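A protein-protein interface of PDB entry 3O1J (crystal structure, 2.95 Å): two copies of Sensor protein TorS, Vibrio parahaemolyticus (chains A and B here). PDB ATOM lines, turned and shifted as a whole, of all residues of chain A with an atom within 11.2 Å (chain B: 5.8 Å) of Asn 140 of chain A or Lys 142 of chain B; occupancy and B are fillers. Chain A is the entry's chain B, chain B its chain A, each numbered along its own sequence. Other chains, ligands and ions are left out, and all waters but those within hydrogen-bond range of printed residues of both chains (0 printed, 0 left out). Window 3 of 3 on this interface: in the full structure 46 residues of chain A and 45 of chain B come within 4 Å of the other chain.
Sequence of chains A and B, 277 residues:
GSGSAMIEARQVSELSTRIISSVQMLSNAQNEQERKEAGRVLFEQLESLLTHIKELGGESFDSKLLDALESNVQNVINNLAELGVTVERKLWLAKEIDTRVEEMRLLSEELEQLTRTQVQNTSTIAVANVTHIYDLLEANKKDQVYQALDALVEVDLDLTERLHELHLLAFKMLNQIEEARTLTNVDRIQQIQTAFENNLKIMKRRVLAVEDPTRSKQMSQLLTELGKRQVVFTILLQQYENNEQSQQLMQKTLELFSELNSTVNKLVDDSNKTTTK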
ATOM      1  N   HIS A 132      33.985 -24.499  25.955  1.00  0.00           N
ATOM      2  CA  HIS A 132      33.061 -23.453  25.542  1.00  0.00           C
ATOM      3  C   HIS A 132      32.598 -23.612  24.114  1.00  0.00           C
ATOM      4  O   HIS A 132      31.466 -23.272  23.788  1.00  0.00           O
ATOM      5  CB  HIS A 132      33.711 -22.089  25.720  1.00  0.00           C
ATOM      6  CG  HIS A 132      32.817 -20.943  25.381  1.00  0.00           C
ATOM      7  ND1 HIS A 132      32.728 -20.419  24.110  1.00  0.00           N
ATOM      8  CD2 HIS A 132      32.003 -20.188  26.154  1.00  0.00           C
ATOM      9  CE1 HIS A 132      31.906 -19.387  24.114  1.00  0.00           C
ATOM     10  NE2 HIS A 132      31.452 -19.226  25.344  1.00  0.00           N
ATOM     11  N   ILE A 133      33.466 -24.120  23.252  1.00  0.00           N
ATOM     12  CA  ILE A 133      33.069 -24.301  21.874  1.00  0.00           C
ATOM     13  C   ILE A 133      31.928 -25.303  21.833  1.00  0.00           C
ATOM     14  O   ILE A 133      30.997 -25.141  21.060  1.00  0.00           O
ATOM     15  CB  ILE A 133      34.246 -24.779  21.001  1.00  0.00           C
ATOM     16  CG1 ILE A 133      35.344 -23.718  21.029  1.00  0.00           C
ATOM     17  CG2 ILE A 133      33.794 -25.003  19.560  1.00  0.00           C
ATOM     18  CD1 ILE A 133      36.474 -23.977  20.079  1.00  0.00           C
ATOM     19  N   TYR A 134      31.977 -26.326  22.676  1.00  0.00           N
ATOM     20  CA  TYR A 134      30.900 -27.311  22.697  1.00  0.00           C
ATOM     21  C   TYR A 134      29.542 -26.626  22.825  1.00  0.00           C
ATOM     22  O   TYR A 134      28.586 -27.020  22.158  1.00  0.00           O
ATOM     23  CB  TYR A 134      31.064 -28.286  23.860  1.00  0.00           C
ATOM     24  CG  TYR A 134      32.170 -29.294  23.687  1.00  0.00           C
ATOM     25  CD1 TYR A 134      33.216 -29.360  24.602  1.00  0.00           C
ATOM     26  CD2 TYR A 134      32.158 -30.211  22.635  1.00  0.00           C
ATOM     27  CE1 TYR A 134      34.224 -30.316  24.482  1.00  0.00           C
ATOM     28  CE2 TYR A 134      33.167 -31.176  22.508  1.00  0.00           C
ATOM     29  CZ  TYR A 134      34.191 -31.220  23.441  1.00  0.00           C
ATOM     30  OH  TYR A 134      35.169 -32.183  23.373  1.00  0.00           O
ATOM     31  N   ASP A 135      29.460 -25.604  23.679  1.00  0.00           N
ATOM     32  CA  ASP A 135      28.207 -24.874  23.902  1.00  0.00           C
ATOM     33  C   ASP A 135      27.747 -24.156  22.653  1.00  0.00           C
ATOM     34  O   ASP A 135      26.634 -24.375  22.179  1.00  0.00           O
ATOM     35  CB  ASP A 135      28.365 -23.854  25.030  1.00  0.00           C
ATOM     36  CG  ASP A 135      28.665 -24.506  26.372  1.00  0.00           C
ATOM     37  OD1 ASP A 135      28.927 -23.767  27.355  1.00  0.00           O
ATOM     38  OD2 ASP A 135      28.637 -25.762  26.442  1.00  0.00           O
ATOM     39  N   LEU A 136      28.599 -23.286  22.131  1.00  0.00           N
ATOM     40  CA  LEU A 136      28.273 -22.561  20.917  1.00  0.00           C
ATOM     41  C   LEU A 136      27.826 -23.588  19.865  1.00  0.00           C
ATOM     42  O   LEU A 136      26.717 -23.520  19.340  1.00  0.00           O
ATOM     43  CB  LEU A 136      29.507 -21.813  20.401  1.00  0.00           C
ATOM     44  CG  LEU A 136      30.278 -20.913  21.368  1.00  0.00           C
ATOM     45  CD1 LEU A 136      31.580 -20.489  20.732  1.00  0.00           C
ATOM     46  CD2 LEU A 136      29.447 -19.707  21.725  1.00  0.00           C
ATOM     47  N   LEU A 137      28.700 -24.550  19.581  1.00  0.00           N
ATOM     48  CA  LEU A 137      28.435 -25.587  18.590  1.00  0.00           C
ATOM     49  C   LEU A 137      27.042 -26.171  18.732  1.00  0.00           C
ATOM     50  O   LEU A 137      26.322 -26.325  17.746  1.00  0.00           O
ATOM     51  CB  LEU A 137      29.496 -26.693  18.704  1.00  0.00           C
ATOM     52  CG  LEU A 137      29.584 -27.860  17.712  1.00  0.00           C
ATOM     53  CD1 LEU A 137      28.602 -28.933  18.101  1.00  0.00           C
ATOM     54  CD2 LEU A 137      29.341 -27.372  16.294  1.00  0.00           C
ATOM     55  N   GLU A 138      26.648 -26.485  19.958  1.00  0.00           N
ATOM     56  CA  GLU A 138      25.333 -27.066  20.162  1.00  0.00           C
ATOM     57  C   GLU A 138      24.325 -26.047  20.675  1.00  0.00           C
ATOM     58  O   GLU A 138      23.768 -26.183  21.762  1.00  0.00           O
ATOM     59  CB  GLU A 138      25.425 -28.248  21.121  1.00  0.00           C
ATOM     60  CG  GLU A 138      24.332 -29.273  20.888  1.00  0.00           C
ATOM     61  CD  GLU A 138      23.860 -29.906  22.176  1.00  0.00           C
ATOM     62  OE1 GLU A 138      23.451 -29.199  23.107  1.00  0.00           O
ATOM     63  OE2 GLU A 138      23.905 -31.242  22.244  1.00  0.00           O
ATOM     64  N   ALA A 139      24.113 -25.027  19.856  1.00  0.00           N
ATOM     65  CA  ALA A 139      23.199 -23.918  20.104  1.00  0.00           C
ATOM     66  C   ALA A 139      23.275 -23.224  18.762  1.00  0.00           C
ATOM     67  O   ALA A 139      22.893 -22.068  18.602  1.00  0.00           O
ATOM     68  CB  ALA A 139      23.728 -23.007  21.200  1.00  0.00           C
ATOM     69  N   ASN A 140      23.832 -23.970  17.813  1.00  0.00           N
ATOM     70  CA  ASN A 140      24.016 -23.562  16.429  1.00  0.00           C
ATOM     71  C   ASN A 140      24.489 -22.137  16.190  1.00  0.00           C
ATOM     72  O   ASN A 140      24.072 -21.503  15.221  1.00  0.00           O
ATOM     73  CB  ASN A 140      22.722 -23.820  15.668  1.00  0.00           C
ATOM     74  CG  ASN A 140      22.191 -25.219  15.903  1.00  0.00           C
ATOM     75  OD1 ASN A 140      22.754 -26.208  15.415  1.00  0.00           O
ATOM     76  ND2 ASN A 140      21.116 -25.316  16.679  1.00  0.00           N
ATOM     77  N   LYS A 141      25.367 -21.638  17.056  1.00  0.00           N
ATOM     78  CA  LYS A 141      25.893 -20.284  16.907  1.00  0.00           C
ATOM     79  C   LYS A 141      27.011 -20.272  15.868  1.00  0.00           C
ATOM     80  O   LYS A 141      27.921 -19.447  15.931  1.00  0.00           O
ATOM     81  CB  LYS A 141      26.425 -19.763  18.242  1.00  0.00           C
ATOM     82  CG  LYS A 141      25.361 -19.449  19.294  1.00  0.00           C
ATOM     83  CD  LYS A 141      26.034 -19.003  20.598  1.00  0.00           C
ATOM     84  CE  LYS A 141      25.042 -18.533  21.653  1.00  0.00           C
ATOM     85  NZ  LYS A 141      24.378 -17.260  21.266  1.00  0.00           N
ATOM     86  N   LYS A 142      26.913 -21.192  14.912  1.00  0.00           N
ATOM     87  CA  LYS A 142      27.875 -21.359  13.824  1.00  0.00           C
ATOM     88  C   LYS A 142      28.976 -20.311  13.648  1.00  0.00           C
ATOM     89  O   LYS A 142      30.149 -20.618  13.827  1.00  0.00           O
ATOM     90  CB  LYS A 142      27.129 -21.514  12.496  1.00  0.00           C
ATOM     91  CG  LYS A 142      28.035 -21.501  11.271  1.00  0.00           C
ATOM     92  CD  LYS A 142      28.199 -22.874  10.654  1.00  0.00           C
ATOM     93  CE  LYS A 142      26.932 -23.337   9.968  1.00  0.00           C
ATOM     94  NZ  LYS A 142      27.220 -24.438   9.011  1.00  0.00           N
ATOM     95  N   ASP A 143      28.619 -19.086  13.281  1.00  0.00           N
ATOM     96  CA  ASP A 143      29.639 -18.066  13.067  1.00  0.00           C
ATOM     97  C   ASP A 143      30.606 -17.872  14.216  1.00  0.00           C
ATOM     98  O   ASP A 143      31.762 -17.525  14.002  1.00  0.00           O
ATOM     99  CB  ASP A 143      29.006 -16.726  12.712  1.00  0.00           C
ATOM    100  CG  ASP A 143      29.066 -16.443  11.218  1.00  0.00           C
ATOM    101  OD1 ASP A 143      30.191 -16.415  10.656  1.00  0.00           O
ATOM    102  OD2 ASP A 143      27.987 -16.254  10.606  1.00  0.00           O
ATOM    103  N   GLN A 144      30.142 -18.098  15.435  1.00  0.00           N
ATOM    104  CA  GLN A 144      31.004 -17.936  16.593  1.00  0.00           C
ATOM    105  C   GLN A 144      31.806 -19.194  16.846  1.00  0.00           C
ATOM    106  O   GLN A 144      32.914 -19.128  17.362  1.00  0.00           O
ATOM    107  CB  GLN A 144      30.165 -17.600  17.808  1.00  0.00           C
ATOM    108  CG  GLN A 144      29.274 -16.416  17.563  1.00  0.00           C
ATOM    109  CD  GLN A 144      28.170 -16.326  18.578  1.00  0.00           C
ATOM    110  OE1 GLN A 144      28.421 -16.151  19.776  1.00  0.00           O
ATOM    111  NE2 GLN A 144      26.929 -16.452  18.109  1.00  0.00           N
ATOM    112  N   VAL A 145      31.243 -20.342  16.489  1.00  0.00           N
ATOM    113  CA  VAL A 145      31.953 -21.596  16.673  1.00  0.00           C
ATOM    114  C   VAL A 145      33.278 -21.504  15.960  1.00  0.00           C
ATOM    115  O   VAL A 145      34.319 -21.758  16.555  1.00  0.00           O
ATOM    116  CB  VAL A 145      31.194 -22.788  16.103  1.00  0.00           C
ATOM    117  CG1 VAL A 145      32.093 -24.011  16.083  1.00  0.00           C
ATOM    118  CG2 VAL A 145      29.971 -23.048  16.940  1.00  0.00           C
ATOM    119  N   TYR A 146      33.270 -21.158  14.679  1.00  0.00           N
ATOM    120  CA  TYR A 146      34.557 -21.057  14.037  1.00  0.00           C
ATOM    121  C   TYR A 146      35.048 -19.641  13.928  1.00  0.00           C
ATOM    122  O   TYR A 146      35.184 -19.071  12.860  1.00  0.00           O
ATOM    123  CB  TYR A 146      34.635 -21.829  12.697  1.00  0.00           C
ATOM    124  CG  TYR A 146      33.796 -21.445  11.486  1.00  0.00           C
ATOM    125  CD1 TYR A 146      33.308 -20.164  11.303  1.00  0.00           C
ATOM    126  CD2 TYR A 146      33.635 -22.371  10.440  1.00  0.00           C
ATOM    127  CE1 TYR A 146      32.699 -19.813  10.114  1.00  0.00           C
ATOM    128  CE2 TYR A 146      33.035 -22.037   9.259  1.00  0.00           C
ATOM    129  CZ  TYR A 146      32.573 -20.757   9.094  1.00  0.00           C
ATOM    130  OH  TYR A 146      32.025 -20.399   7.886  1.00  0.00           O
ATOM    131  N   LEU A 149      37.429 -21.234  16.979  1.00  0.00           N
ATOM    132  CA  LEU A 149      38.389 -22.150  16.399  1.00  0.00           C
ATOM    133  C   LEU A 149      39.583 -21.324  15.955  1.00  0.00           C
ATOM    134  O   LEU A 149      40.722 -21.744  16.115  1.00  0.00           O
ATOM    135  CB  LEU A 149      37.788 -22.885  15.207  1.00  0.00           C
ATOM    136  CG  LEU A 149      36.777 -23.961  15.590  1.00  0.00           C
ATOM    137  CD1 LEU A 149      36.308 -24.677  14.338  1.00  0.00           C
ATOM    138  CD2 LEU A 149      37.412 -24.950  16.553  1.00  0.00           C
ATOM    139  N   LEU B 136      33.981 -29.524   8.419  1.00  0.00           N
ATOM    140  CA  LEU B 136      32.875 -30.231   9.053  1.00  0.00           C
ATOM    141  C   LEU B 136      31.834 -29.244   9.551  1.00  0.00           C
ATOM    142  O   LEU B 136      30.664 -29.328   9.199  1.00  0.00           O
ATOM    143  CB  LEU B 136      33.378 -31.061  10.237  1.00  0.00           C
ATOM    144  CG  LEU B 136      34.244 -32.267   9.901  1.00  0.00           C
ATOM    145  CD1 LEU B 136      34.582 -33.026  11.158  1.00  0.00           C
ATOM    146  CD2 LEU B 136      33.487 -33.156   8.943  1.00  0.00           C
ATOM    147  N   ALA B 139      29.400 -27.636   7.027  1.00  0.00           N
ATOM    148  CA  ALA B 139      28.863 -28.688   6.171  1.00  0.00           C
ATOM    149  C   ALA B 139      27.836 -29.310   7.106  1.00  0.00           C
ATOM    150  O   ALA B 139      27.312 -30.399   6.873  1.00  0.00           O
ATOM    151  CB  ALA B 139      29.937 -29.702   5.810  1.00  0.00           C
ATOM    152  N   ASN B 140      27.594 -28.577   8.191  1.00  0.00           N
ATOM    153  CA  ASN B 140      26.648 -28.923   9.241  1.00  0.00           C
ATOM    154  C   ASN B 140      26.656 -30.362   9.722  1.00  0.00           C
ATOM    155  O   ASN B 140      25.609 -30.905  10.071  1.00  0.00           O
ATOM    156  CB  ASN B 140      25.246 -28.527   8.800  1.00  0.00           C
ATOM    157  CG  ASN B 140      25.159 -27.062   8.427  1.00  0.00           C
ATOM    158  OD1 ASN B 140      25.389 -26.184   9.266  1.00  0.00           O
ATOM    159  ND2 ASN B 140      24.841 -26.783   7.158  1.00  0.00           N
ATOM    160  N   LYS B 141      27.836 -30.976   9.745  1.00  0.00           N
ATOM    161  CA  LYS B 141      27.981 -32.344  10.230  1.00  0.00           C
ATOM    162  C   LYS B 141      28.144 -32.249  11.748  1.00  0.00           C
ATOM    163  O   LYS B 141      28.963 -32.946  12.338  1.00  0.00           O
ATOM    164  CB  LYS B 141      29.221 -33.009   9.621  1.00  0.00           C
ATOM    165  CG  LYS B 141      29.148 -33.331   8.122  1.00  0.00           C
ATOM    166  CD  LYS B 141      30.496 -33.893   7.630  1.00  0.00           C
ATOM    167  CE  LYS B 141      30.475 -34.395   6.181  1.00  0.00           C
ATOM    168  NZ  LYS B 141      30.111 -35.842   6.056  1.00  0.00           N
ATOM    169  N   LYS B 142      27.350 -31.371  12.358  1.00  0.00           N
ATOM    170  CA  LYS B 142      27.363 -31.113  13.799  1.00  0.00           C
ATOM    171  C   LYS B 142      27.898 -32.204  14.730  1.00  0.00           C
ATOM    172  O   LYS B 142      28.617 -31.894  15.675  1.00  0.00           O
ATOM    173  CB  LYS B 142      25.964 -30.692  14.264  1.00  0.00           C
ATOM    174  CG  LYS B 142      25.731 -30.859  15.754  1.00  0.00           C
ATOM    175  CD  LYS B 142      25.488 -29.537  16.482  1.00  0.00           C
ATOM    176  CE  LYS B 142      24.096 -28.964  16.221  1.00  0.00           C
ATOM    177  NZ  LYS B 142      23.691 -27.970  17.261  1.00  0.00           N
ATOM    178  N   ASP B 143      27.566 -33.468  14.492  1.00  0.00           N
ATOM    179  CA  ASP B 143      28.060 -34.517  15.383  1.00  0.00           C
ATOM    180  C   ASP B 143      29.536 -34.828  15.241  1.00  0.00           C
ATOM    181  O   ASP B 143      30.204 -35.137  16.221  1.00  0.00           O
ATOM    182  CB  ASP B 143      27.256 -35.807  15.217  1.00  0.00           C
ATOM    183  CG  ASP B 143      25.880 -35.719  15.857  1.00  0.00           C
ATOM    184  OD1 ASP B 143      25.796 -35.253  17.025  1.00  0.00           O
ATOM    185  OD2 ASP B 143      24.889 -36.119  15.195  1.00  0.00           O
ATOM    186  N   GLN B 144      30.052 -34.755  14.023  1.00  0.00           N
ATOM    187  CA  GLN B 144      31.460 -35.024  13.811  1.00  0.00           C
ATOM    188  C   GLN B 144      32.296 -33.868  14.335  1.00  0.00           C
ATOM    189  O   GLN B 144      33.483 -34.038  14.610  1.00  0.00           O
ATOM    190  CB  GLN B 144      31.729 -35.240  12.334  1.00  0.00           C
ATOM    191  CG  GLN B 144      30.909 -36.363  11.757  1.00  0.00           C
ATOM    192  CD  GLN B 144      31.118 -36.511  10.271  1.00  0.00           C
ATOM    193  OE1 GLN B 144      32.230 -36.786   9.813  1.00  0.00           O
ATOM    194  NE2 GLN B 144      30.049 -36.326   9.503  1.00  0.00           N
ATOM    195  N   VAL B 145      31.680 -32.693  14.461  1.00  0.00           N
ATOM    196  CA  VAL B 145      32.385 -31.535  14.986  1.00  0.00           C
ATOM    197  C   VAL B 145      32.719 -31.867  16.428  1.00  0.00           C
ATOM    198  O   VAL B 145      33.873 -32.174  16.708  1.00  0.00           O
ATOM    199  CB  VAL B 145      31.554 -30.244  14.898  1.00  0.00           C
ATOM    200  CG1 VAL B 145      32.250 -29.122  15.634  1.00  0.00           C
ATOM    201  CG2 VAL B 145      31.392 -29.853  13.453  1.00  0.00           C
ATOM    202  N   TYR B 146      31.772 -31.823  17.365  1.00  0.00           N
ATOM    203  CA  TYR B 146      32.211 -32.209  18.704  1.00  0.00           C
ATOM    204  C   TYR B 146      32.339 -33.697  18.724  1.00  0.00           C
ATOM    205  O   TYR B 146      31.423 -34.410  19.084  1.00  0.00           O
ATOM    206  CB  TYR B 146      31.327 -31.729  19.886  1.00  0.00           C
ATOM    207  CG  TYR B 146      29.813 -31.777  19.824  1.00  0.00           C
ATOM    208  CD1 TYR B 146      29.136 -32.683  19.029  1.00  0.00           C
ATOM    209  CD2 TYR B 146      29.065 -30.888  20.611  1.00  0.00           C
ATOM    210  CE1 TYR B 146      27.752 -32.698  19.012  1.00  0.00           C
ATOM    211  CE2 TYR B 146      27.698 -30.892  20.606  1.00  0.00           C
ATOM    212  CZ  TYR B 146      27.039 -31.793  19.805  1.00  0.00           C
ATOM    213  OH  TYR B 146      25.661 -31.772  19.779  1.00  0.00           O
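The side-chain amide oxygen of Asn 140 of chain B sits at hydrogen-bond distance from the side-chain amino group of Lys 142 of chain A (2.5 Å). NZ of Lys 142 of chain B sits at hydrogen-bond distance from O of Leu 137 of chain A (3.1 Å). The side-chain amino group of Lys 142 of chain B is in hydrogen-bond range of the side-chain amide oxygen of Asn 140 of chain A (2.7 Å). OE2 of Glu 138 of chain A lies close to OH of Tyr 146 of chain B, 3.1 Å away.
Among the printed residues, merely in contact across the chains: Tyr 134 of chain A with Tyr 146 of chain B, Leu 137 of chain A with Val 145 of chain B, Leu 137 of chain A with Tyr 146 of chain B, Glu 138 of chain A with Lys 142 of chain B and Ala 139 of chain A with Lys 142 of chain B.
Of the printed residues of chain B, Tyr 134 of chain A touches Tyr 146. Printed residues of chain B within 4 Å of Leu 137 of chain A: Lys 142 (3.1 Å), Val 145 (3.5 Å) and Tyr 146 (3.2 Å). Of the printed residues of chain B, Glu 138 of chain A touches Lys 142 (3.5 Å) and Tyr 146 (3.0 Å). Of the printed residues of chain B, Lys 142 of chain A touches Asn 140. Of the printed residues of chain A, Asn 140 of chain B touches Lys 142 (2.5 Å). Lys 141 of chain B touches none of the printed residues of chain A. Printed residues of chain A within 4 Å of Lys 142 of chain B: Leu 137 (3.1 Å), Glu 138 (3.5 Å), Ala 139 (3.9 Å) and Asn 140 (2.7 Å). No residue of chain A comes within 4 Å of Asp 143 of chain B. Printed residues of chain A within 4 Å of Tyr 146 of chain B: Tyr 134 (3.2 Å), Leu 137 (3.2 Å) and Glu 138 (3.0 Å).
Printed residues of chain A that touch a printed residue of chain B: Tyr 134, Leu 137, Glu 138, Ala 139, Asn 140 and Lys 142. Hydrophobic or aromatic side chains of chain A that line the printed part of chain B: Tyr 134 and Leu 137. Among the printed residues, 9 pairs touch across the chains. Among the printed residues, no Asp or Glu carboxylate lies within 4 Å of a Lys or Arg side-chain nitrogen of the other chain.
Ala 139 of chain A touches Lys 142 of chain B, but with the chains exchanged Lys 142 of chain A does not touch Ala 139 of chain B (4.3 Å). Asn 140 of chain A touches Lys 142 of chain B, and with the chains exchanged Lys 142 of chain A touches Asn 140 of chain B.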
